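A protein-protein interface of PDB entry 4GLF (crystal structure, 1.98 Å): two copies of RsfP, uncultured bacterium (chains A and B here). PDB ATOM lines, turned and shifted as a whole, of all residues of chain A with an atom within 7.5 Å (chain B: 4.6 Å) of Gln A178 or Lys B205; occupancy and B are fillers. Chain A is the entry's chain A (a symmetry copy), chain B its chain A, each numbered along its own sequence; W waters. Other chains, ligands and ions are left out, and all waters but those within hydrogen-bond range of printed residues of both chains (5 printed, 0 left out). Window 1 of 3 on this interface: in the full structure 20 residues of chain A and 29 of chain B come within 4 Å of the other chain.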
ATOM      1  N   LYS A 122      -0.944  21.817 -20.928  1.00  0.00           N
ATOM      2  CA  LYS A 122      -0.007  22.770 -21.556  1.00  0.00           C
ATOM      3  C   LYS A 122       0.063  22.691 -23.087  1.00  0.00           C
ATOM      4  O   LYS A 122       0.199  23.712 -23.771  1.00  0.00           O
ATOM      5  CB  LYS A 122       1.391  22.455 -20.962  1.00  0.00           C
ATOM      6  CG  LYS A 122       1.533  22.836 -19.473  1.00  0.00           C
ATOM      7  CD  LYS A 122       2.564  21.968 -18.739  1.00  0.00           C
ATOM      8  CE  LYS A 122       2.758  22.296 -17.228  1.00  0.00           C
ATOM      9  NZ  LYS A 122       4.197  21.907 -16.800  1.00  0.00           N
ATOM     10  N   ILE A 174      -4.273  17.878 -15.578  1.00  0.00           N
ATOM     11  CA  ILE A 174      -2.833  18.158 -15.757  1.00  0.00           C
ATOM     12  C   ILE A 174      -2.357  17.516 -17.078  1.00  0.00           C
ATOM     13  O   ILE A 174      -3.058  16.704 -17.675  1.00  0.00           O
ATOM     14  CB  ILE A 174      -1.951  17.695 -14.541  1.00  0.00           C
ATOM     15  CG1 ILE A 174      -2.040  16.146 -14.378  1.00  0.00           C
ATOM     16  CG2 ILE A 174      -2.352  18.432 -13.264  1.00  0.00           C
ATOM     17  CD1 ILE A 174      -1.004  15.599 -13.399  1.00  0.00           C
ATOM     18  N   GLU A 175      -1.179  17.935 -17.559  1.00  0.00           N
ATOM     19  CA  GLU A 175      -0.684  17.447 -18.827  1.00  0.00           C
ATOM     20  C   GLU A 175      -0.346  15.952 -18.782  1.00  0.00           C
ATOM     21  O   GLU A 175      -0.579  15.286 -19.709  1.00  0.00           O
ATOM     22  CB  GLU A 175       0.576  18.257 -19.270  1.00  0.00           C
ATOM     23  CG  GLU A 175       1.086  17.899 -20.682  1.00  0.00           C
ATOM     24  CD  GLU A 175      -0.035  18.109 -21.741  1.00  0.00           C
ATOM     25  OE1 GLU A 175      -0.584  19.218 -21.757  1.00  0.00           O
ATOM     26  OE2 GLU A 175      -0.420  17.178 -22.532  1.00  0.00           O
ATOM     27  N   GLY A 176       0.267  15.483 -17.700  1.00  0.00           N
ATOM     28  CA  GLY A 176       0.864  14.153 -17.644  1.00  0.00           C
ATOM     29  C   GLY A 176       2.078  14.070 -18.545  1.00  0.00           C
ATOM     30  O   GLY A 176       2.547  15.128 -19.056  1.00  0.00           O
ATOM     31  N   PRO A 177       2.552  12.828 -18.819  1.00  0.00           N
ATOM     32  CA  PRO A 177       1.891  11.554 -18.341  1.00  0.00           C
ATOM     33  C   PRO A 177       2.315  11.149 -16.900  1.00  0.00           C
ATOM     34  O   PRO A 177       1.719  10.210 -16.369  1.00  0.00           O
ATOM     35  CB  PRO A 177       2.381  10.504 -19.332  1.00  0.00           C
ATOM     36  CG  PRO A 177       3.835  10.966 -19.576  1.00  0.00           C
ATOM     37  CD  PRO A 177       3.728  12.536 -19.661  1.00  0.00           C
ATOM     38  N   GLN A 178       3.298  11.845 -16.286  1.00  0.00           N
ATOM     39  CA  GLN A 178       3.681  11.440 -14.921  1.00  0.00           C
ATOM     40  C   GLN A 178       2.686  11.859 -13.872  1.00  0.00           C
ATOM     41  O   GLN A 178       2.020  12.908 -14.014  1.00  0.00           O
ATOM     42  CB  GLN A 178       5.122  11.960 -14.546  1.00  0.00           C
ATOM     43  CG  GLN A 178       6.180  11.568 -15.606  1.00  0.00           C
ATOM     44  CD  GLN A 178       6.305  12.640 -16.708  1.00  0.00           C
ATOM     45  OE1 GLN A 178       5.597  13.672 -16.675  1.00  0.00           O
ATOM     46  NE2 GLN A 178       7.153  12.406 -17.688  1.00  0.00           N
ATOM     47  N   PHE A 179       2.638  11.122 -12.749  1.00  0.00           N
ATOM     48  CA  PHE A 179       1.831  11.584 -11.625  1.00  0.00           C
ATOM     49  C   PHE A 179       2.510  12.742 -10.901  1.00  0.00           C
ATOM     50  O   PHE A 179       3.713  12.986 -11.121  1.00  0.00           O
ATOM     51  CB  PHE A 179       1.454  10.420 -10.673  1.00  0.00           C
ATOM     52  CG  PHE A 179       0.676   9.275 -11.336  1.00  0.00           C
ATOM     53  CD1 PHE A 179      -0.643   9.450 -11.769  1.00  0.00           C
ATOM     54  CD2 PHE A 179       1.245   7.995 -11.462  1.00  0.00           C
ATOM     55  CE1 PHE A 179      -1.380   8.375 -12.329  1.00  0.00           C
ATOM     56  CE2 PHE A 179       0.539   6.919 -12.021  1.00  0.00           C
ATOM     57  CZ  PHE A 179      -0.796   7.099 -12.448  1.00  0.00           C
ATOM     58  N   SER A 180       1.726  13.519 -10.137  1.00  0.00           N
ATOM     59  CA  SER A 180       2.170  14.796  -9.538  1.00  0.00           C
ATOM     60  C   SER A 180       3.236  14.647  -8.499  1.00  0.00           C
ATOM     61  O   SER A 180       3.294  13.617  -7.785  1.00  0.00           O
ATOM     62  CB  SER A 180       0.932  15.456  -8.862  1.00  0.00           C
ATOM     63  OG  SER A 180       0.049  15.892  -9.900  1.00  0.00           O
ATOM     64  N   THR A 181       4.051  15.682  -8.320  1.00  0.00           N
ATOM     65  CA  THR A 181       4.964  15.668  -7.186  1.00  0.00           C
ATOM     66  C   THR A 181       4.059  15.960  -5.962  1.00  0.00           C
ATOM     67  O   THR A 181       2.922  16.386  -6.133  1.00  0.00           O
ATOM     68  CB  THR A 181       6.063  16.753  -7.333  1.00  0.00           C
ATOM     69  OG1 THR A 181       5.419  18.011  -7.272  1.00  0.00           O
ATOM     70  CG2 THR A 181       6.841  16.686  -8.712  1.00  0.00           C
ATOM     71  N   GLU A 184       3.089  19.662  -5.954  1.00  0.00           N
ATOM     72  CA  GLU A 184       2.064  20.059  -6.901  1.00  0.00           C
ATOM     73  C   GLU A 184       0.724  19.617  -6.280  1.00  0.00           C
ATOM     74  O   GLU A 184      -0.230  20.371  -6.321  1.00  0.00           O
ATOM     75  CB  GLU A 184       2.287  19.370  -8.309  1.00  0.00           C
ATOM     76  CG  GLU A 184       3.501  19.952  -9.067  1.00  0.00           C
ATOM     77  CD  GLU A 184       4.028  19.067 -10.204  1.00  0.00           C
ATOM     78  OE1 GLU A 184       3.552  17.862 -10.393  1.00  0.00           O
ATOM     79  OE2 GLU A 184       4.900  19.625 -10.960  1.00  0.00           O
ATOM     80  N   ILE A 196      -8.025  14.932  -9.486  1.00  0.00           N
ATOM     81  CA  ILE A 196      -7.064  15.238 -10.511  1.00  0.00           C
ATOM     82  C   ILE A 196      -7.137  14.177 -11.611  1.00  0.00           C
ATOM     83  O   ILE A 196      -7.115  12.964 -11.350  1.00  0.00           O
ATOM     84  CB  ILE A 196      -5.638  15.376  -9.915  1.00  0.00           C
ATOM     85  CG1 ILE A 196      -4.606  15.597 -11.065  1.00  0.00           C
ATOM     86  CG2 ILE A 196      -5.240  14.165  -9.044  1.00  0.00           C
ATOM     87  CD1 ILE A 196      -3.400  16.247 -10.448  1.00  0.00           C
ATOM     88  N   MET A 198      -6.137  13.679 -16.252  1.00  0.00           N
ATOM     89  CA  MET A 198      -5.318  14.103 -17.343  1.00  0.00           C
ATOM     90  C   MET A 198      -6.076  14.287 -18.659  1.00  0.00           C
ATOM     91  O   MET A 198      -5.415  14.609 -19.657  1.00  0.00           O
ATOM     92  CB  MET A 198      -4.199  13.044 -17.543  1.00  0.00           C
ATOM     93  CG  MET A 198      -3.311  12.960 -16.324  1.00  0.00           C
ATOM     94  SD  MET A 198      -1.970  11.822 -16.643  1.00  0.00           S
ATOM     95  CE  MET A 198      -1.250  11.806 -15.001  1.00  0.00           C
ATOM     96  N   ASP A 224      -4.148  10.736  -4.814  1.00  0.00           N
ATOM     97  CA  ASP A 224      -2.996  11.442  -5.297  1.00  0.00           C
ATOM     98  C   ASP A 224      -2.041  11.515  -4.092  1.00  0.00           C
ATOM     99  O   ASP A 224      -2.468  11.443  -2.926  1.00  0.00           O
ATOM    100  CB  ASP A 224      -3.409  12.779  -5.881  1.00  0.00           C
ATOM    101  CG  ASP A 224      -2.363  13.345  -6.815  1.00  0.00           C
ATOM    102  OD1 ASP A 224      -2.065  14.552  -6.718  1.00  0.00           O
ATOM    103  OD2 ASP A 224      -1.834  12.572  -7.643  1.00  0.00           O
ATOM    104  N   ASP B 119       6.471  21.822 -11.570  1.00  0.00           N
ATOM    105  CA  ASP B 119       6.833  22.014 -12.969  1.00  0.00           C
ATOM    106  C   ASP B 119       5.912  23.085 -13.565  1.00  0.00           C
ATOM    107  O   ASP B 119       4.777  22.809 -13.854  1.00  0.00           O
ATOM    108  CB  ASP B 119       6.774  20.718 -13.748  1.00  0.00           C
ATOM    109  CG  ASP B 119       7.251  20.866 -15.192  1.00  0.00           C
ATOM    110  OD1 ASP B 119       7.566  22.024 -15.633  1.00  0.00           O
ATOM    111  OD2 ASP B 119       7.266  19.807 -15.938  1.00  0.00           O
ATOM    112  N   SER B 126       8.244  16.606 -22.239  1.00  0.00           N
ATOM    113  CA  SER B 126       8.597  16.233 -20.875  1.00  0.00           C
ATOM    114  C   SER B 126       8.411  14.731 -20.583  1.00  0.00           C
ATOM    115  O   SER B 126       8.280  14.322 -19.420  1.00  0.00           O
ATOM    116  CB  SER B 126       7.805  17.100 -19.918  1.00  0.00           C
ATOM    117  OG  SER B 126       6.441  16.870 -20.101  1.00  0.00           O
ATOM    118  N   THR B 127       8.416  13.911 -21.650  1.00  0.00           N
ATOM    119  CA  THR B 127       8.369  12.444 -21.481  1.00  0.00           C
ATOM    120  C   THR B 127       9.055  11.797 -22.653  1.00  0.00           C
ATOM    121  O   THR B 127       9.171  12.395 -23.744  1.00  0.00           O
ATOM    122  CB  THR B 127       6.873  11.917 -21.415  1.00  0.00           C
ATOM    123  OG1 THR B 127       6.830  10.493 -21.276  1.00  0.00           O
ATOM    124  CG2 THR B 127       6.014  12.292 -22.655  1.00  0.00           C
ATOM    125  N   VAL B 137       5.062   7.250 -14.668  1.00  0.00           N
ATOM    126  CA  VAL B 137       5.883   7.117 -13.476  1.00  0.00           C
ATOM    127  C   VAL B 137       5.374   8.077 -12.391  1.00  0.00           C
ATOM    128  O   VAL B 137       4.684   9.056 -12.674  1.00  0.00           O
ATOM    129  CB  VAL B 137       7.388   7.293 -13.748  1.00  0.00           C
ATOM    130  CG1 VAL B 137       7.802   6.261 -14.808  1.00  0.00           C
ATOM    131  CG2 VAL B 137       7.718   8.742 -14.249  1.00  0.00           C
ATOM    132  N   MET B 139       6.089  10.825  -9.643  1.00  0.00           N
ATOM    133  CA  MET B 139       7.087  11.853  -9.352  1.00  0.00           C
ATOM    134  C   MET B 139       6.810  12.361  -7.929  1.00  0.00           C
ATOM    135  O   MET B 139       7.244  13.453  -7.571  1.00  0.00           O
ATOM    136  CB  MET B 139       6.907  13.003 -10.347  1.00  0.00           C
ATOM    137  CG  MET B 139       7.214  12.572 -11.782  1.00  0.00           C
ATOM    138  SD  MET B 139       8.935  12.066 -11.943  1.00  0.00           S
ATOM    139  CE  MET B 139       9.952  13.467 -11.431  1.00  0.00           C
ATOM    140  N   MET B 201      13.259  20.957 -14.732  1.00  0.00           N
ATOM    141  CA  MET B 201      12.168  20.301 -15.437  1.00  0.00           C
ATOM    142  C   MET B 201      12.291  20.572 -16.896  1.00  0.00           C
ATOM    143  O   MET B 201      12.477  21.752 -17.278  1.00  0.00           O
ATOM    144  CB  MET B 201      10.753  20.758 -14.921  1.00  0.00           C
ATOM    145  CG  MET B 201      10.469  20.184 -13.502  1.00  0.00           C
ATOM    146  SD  MET B 201      10.050  18.386 -13.598  1.00  0.00           S
ATOM    147  CE  MET B 201       9.497  18.099 -11.925  1.00  0.00           C
ATOM    148  N   PRO B 202      12.125  19.533 -17.755  1.00  0.00           N
ATOM    149  CA  PRO B 202      11.685  18.112 -17.497  1.00  0.00           C
ATOM    150  C   PRO B 202      12.828  17.133 -17.135  1.00  0.00           C
ATOM    151  O   PRO B 202      12.566  15.950 -17.041  1.00  0.00           O
ATOM    152  CB  PRO B 202      11.092  17.688 -18.854  1.00  0.00           C
ATOM    153  CG  PRO B 202      11.990  18.441 -19.849  1.00  0.00           C
ATOM    154  CD  PRO B 202      12.258  19.812 -19.207  1.00  0.00           C
ATOM    155  N   GLU B 203      14.027  17.646 -16.881  1.00  0.00           N
ATOM    156  CA  GLU B 203      15.189  16.804 -16.546  1.00  0.00           C
ATOM    157  C   GLU B 203      14.822  15.759 -15.474  1.00  0.00           C
ATOM    158  O   GLU B 203      15.077  14.563 -15.645  1.00  0.00           O
ATOM    159  CB  GLU B 203      16.318  17.716 -16.003  1.00  0.00           C
ATOM    160  CG  GLU B 203      17.579  17.596 -16.761  1.00  0.00           C
ATOM    161  CD  GLU B 203      18.679  18.575 -16.328  1.00  0.00           C
ATOM    162  OE1 GLU B 203      18.893  18.737 -15.099  1.00  0.00           O
ATOM    163  OE2 GLU B 203      19.335  19.166 -17.220  1.00  0.00           O
ATOM    164  N   ALA B 204      14.195  16.191 -14.371  1.00  0.00           N
ATOM    165  CA  ALA B 204      13.855  15.254 -13.325  1.00  0.00           C
ATOM    166  C   ALA B 204      12.821  14.175 -13.748  1.00  0.00           C
ATOM    167  O   ALA B 204      12.928  13.057 -13.288  1.00  0.00           O
ATOM    168  CB  ALA B 204      13.323  15.971 -12.074  1.00  0.00           C
ATOM    169  N   LYS B 205      11.822  14.549 -14.567  1.00  0.00           N
ATOM    170  CA  LYS B 205      10.816  13.622 -15.052  1.00  0.00           C
ATOM    171  C   LYS B 205      11.467  12.557 -15.990  1.00  0.00           C
ATOM    172  O   LYS B 205      11.170  11.341 -15.913  1.00  0.00           O
ATOM    173  CB  LYS B 205       9.750  14.408 -15.866  1.00  0.00           C
ATOM    174  CG  LYS B 205       8.836  15.254 -14.957  1.00  0.00           C
ATOM    175  CD  LYS B 205       7.827  16.016 -15.786  1.00  0.00           C
ATOM    176  CE  LYS B 205       6.826  16.678 -14.809  1.00  0.00           C
ATOM    177  NZ  LYS B 205       5.757  17.541 -15.421  1.00  0.00           N
ATOM    178  N   LEU B 206      12.299  13.036 -16.897  1.00  0.00           N
ATOM    179  CA  LEU B 206      13.000  12.135 -17.840  1.00  0.00           C
ATOM    180  C   LEU B 206      13.938  11.185 -17.117  1.00  0.00           C
ATOM    181  O   LEU B 206      13.991   9.969 -17.473  1.00  0.00           O
ATOM    182  CB  LEU B 206      13.714  12.946 -18.954  1.00  0.00           C
ATOM    183  CG  LEU B 206      12.653  13.720 -19.790  1.00  0.00           C
ATOM    184  CD1 LEU B 206      13.354  14.811 -20.589  1.00  0.00           C
ATOM    185  CD2 LEU B 206      11.922  12.787 -20.764  1.00  0.00           C
ATOM    186  N   ALA B 207      14.686  11.712 -16.132  1.00  0.00           N
ATOM    187  CA  ALA B 207      15.637  10.882 -15.403  1.00  0.00           C
ATOM    188  C   ALA B 207      14.837   9.775 -14.682  1.00  0.00           C
ATOM    189  O   ALA B 207      15.317   8.583 -14.599  1.00  0.00           O
ATOM    190  CB  ALA B 207      16.493  11.719 -14.380  1.00  0.00           C
ATOM    191  N   ARG B 208      13.652  10.133 -14.145  1.00  0.00           N
ATOM    192  CA  ARG B 208      12.799   9.141 -13.465  1.00  0.00           C
ATOM    193  C   ARG B 208      12.344   8.015 -14.437  1.00  0.00           C
ATOM    194  O   ARG B 208      12.453   6.793 -14.126  1.00  0.00           O
ATOM    195  CB  ARG B 208      11.589   9.786 -12.752  1.00  0.00           C
ATOM    196  CG  ARG B 208      10.748   8.813 -11.934  1.00  0.00           C
ATOM    197  CD  ARG B 208      11.459   8.033 -10.788  1.00  0.00           C
ATOM    198  NE  ARG B 208      12.230   8.923  -9.888  1.00  0.00           N
ATOM    199  CZ  ARG B 208      11.731   9.551  -8.816  1.00  0.00           C
ATOM    200  NH1 ARG B 208      10.474   9.365  -8.472  1.00  0.00           N
ATOM    201  NH2 ARG B 208      12.500  10.335  -8.055  1.00  0.00           N
ATOM    202  N   GLU B 209      11.913   8.424 -15.611  1.00  0.00           N
ATOM    203  CA  GLU B 209      11.522   7.478 -16.666  1.00  0.00           C
ATOM    204  C   GLU B 209      12.653   6.581 -17.098  1.00  0.00           C
ATOM    205  O   GLU B 209      12.400   5.445 -17.574  1.00  0.00           O
ATOM    206  CB  GLU B 209      10.992   8.186 -17.903  1.00  0.00           C
ATOM    207  CG  GLU B 209       9.571   8.784 -17.616  1.00  0.00           C
ATOM    208  CD  GLU B 209       8.962   9.519 -18.809  1.00  0.00           C
ATOM    209  OE1 GLU B 209       9.679   9.713 -19.789  1.00  0.00           O
ATOM    210  OE2 GLU B 209       7.735   9.879 -18.819  1.00  0.00           O
HETATM  211  O   HOH W   1       5.002  16.062 -17.812  1.00  0.00           O
HETATM  212  O   HOH W   2       4.058  19.035 -17.233  1.00  0.00           O
HETATM  213  O   HOH W   3       4.154  18.601 -13.783  1.00  0.00           O
HETATM  214  O   HOH W   4       3.201  15.367 -14.635  1.00  0.00           O
HETATM  215  O   HOH W   5       3.529  10.881  -8.282  1.00  0.00           O
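OD1 of Asp B119 is in salt-bridge range of NZ of Lys A122, at 3.6 Å.
N of Asp B119 sits at hydrogen-bond distance from OE2 of Glu A184 (2.8 Å).
NE2 of Gln A178 lies within hydrogen-bond range of OE2 of Glu B209, 2.8 Å away.
The backbone carbonyl oxygen (O) of Val B137 sits at hydrogen-bond distance from the backbone NH (N) of Phe A179 (2.9 Å).
The side-chain amide nitrogen of Gln A178 lies within hydrogen-bond range of the backbone carbonyl oxygen of Ser B126 (2.8 Å).
The side-chain carboxylate of Asp B119 lies within salt-bridge range of the side-chain amino group of Lys B205 (2.8 Å).
The side-chain carboxylate (OE2) of Glu B209 sits at hydrogen-bond distance from the side-chain hydroxyl (OG1) of Thr B127 (2.7 Å).
N of Thr A181 sits at hydrogen-bond distance from OE1 of Glu A184, at 3.0 Å.
The side-chain carboxylate of Glu A175 lies within hydrogen-bond range of the backbone NH of Lys A122, 2.8 Å away.
Among the printed residues, pairs that only touch across the chains: Pro A177 with Thr B127 (3.5 Å), Gln A178 with Thr B127 (3.8 Å), Gln A178 with Val B137 (3.4 Å), Gln A178 with Met B139 (3.5 Å), Gln A178 with Lys B205 (3.4 Å), Phe A179 with Met B139 (3.3 Å), Ser A180 with Met B139 (3.7 Å) and Thr A181 with Met B139 (3.2 Å).
Of chain B, only Ser B126 (2.8 Å), Thr B127 (3.8 Å), Val B137 (3.4 Å), Met B139 (3.5 Å), Lys B205 (3.4 Å) and Glu B209 (2.8 Å) come within 4 Å of Gln A178.
Of chain A, only Gln A178 comes within 4 Å of Lys B205.
Of the printed residues of chain B, Lys A122 touches Asp B119.
Of the printed residues of chain B, Thr A181 touches Met B139.
Of the printed residues of chain A, Val B137 touches Gln A178 (3.4 Å) and Phe A179 (2.9 Å).
Printed residues of chain A within 4 Å of Ser B126: Gln A178.
Ile A196 touches none of the printed residues of chain B.
Met A198 touches none of the printed residues of chain B.
The nearest residue of chain A that does not touch Lys B205 is Lys A122 (4.8 Å).
Of the 14 printed residues of chain B, 7 touch a printed residue of chain A.
Hydrophobic or aromatic side chains of chain B within 4 Å of the printed part of chain A: Val B137 and Met B139.
Of the 13 printed residues of chain A, 7 touch a printed residue of chain B.
Hydrophobic or aromatic side chains of chain A that line the printed part of chain B: Pro A177 and Phe A179.
Along chain A the printed residues that touch a printed residue of chain B span positions 122 to 184.
Among the printed residues, Asp or Glu carboxylates within 4 Å of a Lys or Arg side-chain nitrogen of the other chain: Lys A122 with Asp B119.
No position is printed for both chains.
Of the 13 pairs that touch across the chains among the printed residues, none has its exchanged pair printed and touching as well.
Water W3 bridges the side-chain amino group (NZ) of Lys B205 (2.5 Å) and the side-chain carboxylate (OE2) of Glu A184 (3.1 Å).
Water W1 lies within hydrogen-bond range of OE1 of Gln A178 (2.7 Å), OG of Ser B126 (2.8 Å), O of Gly A176 (2.9 Å) and NZ of Lys B205 (2.9 Å).
Water W5 lies within hydrogen-bond range of O of Ser A180 (2.8 Å) and N of Met B139 (2.9 Å).
Water W4 lies within hydrogen-bond range of O of Gln A178 (2.8 Å) and NZ of Lys B205 (3.4 Å).
Water W2 lies within hydrogen-bond range of NZ of Lys B205 (2.9 Å) and NZ of Lys A122 (2.9 Å).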
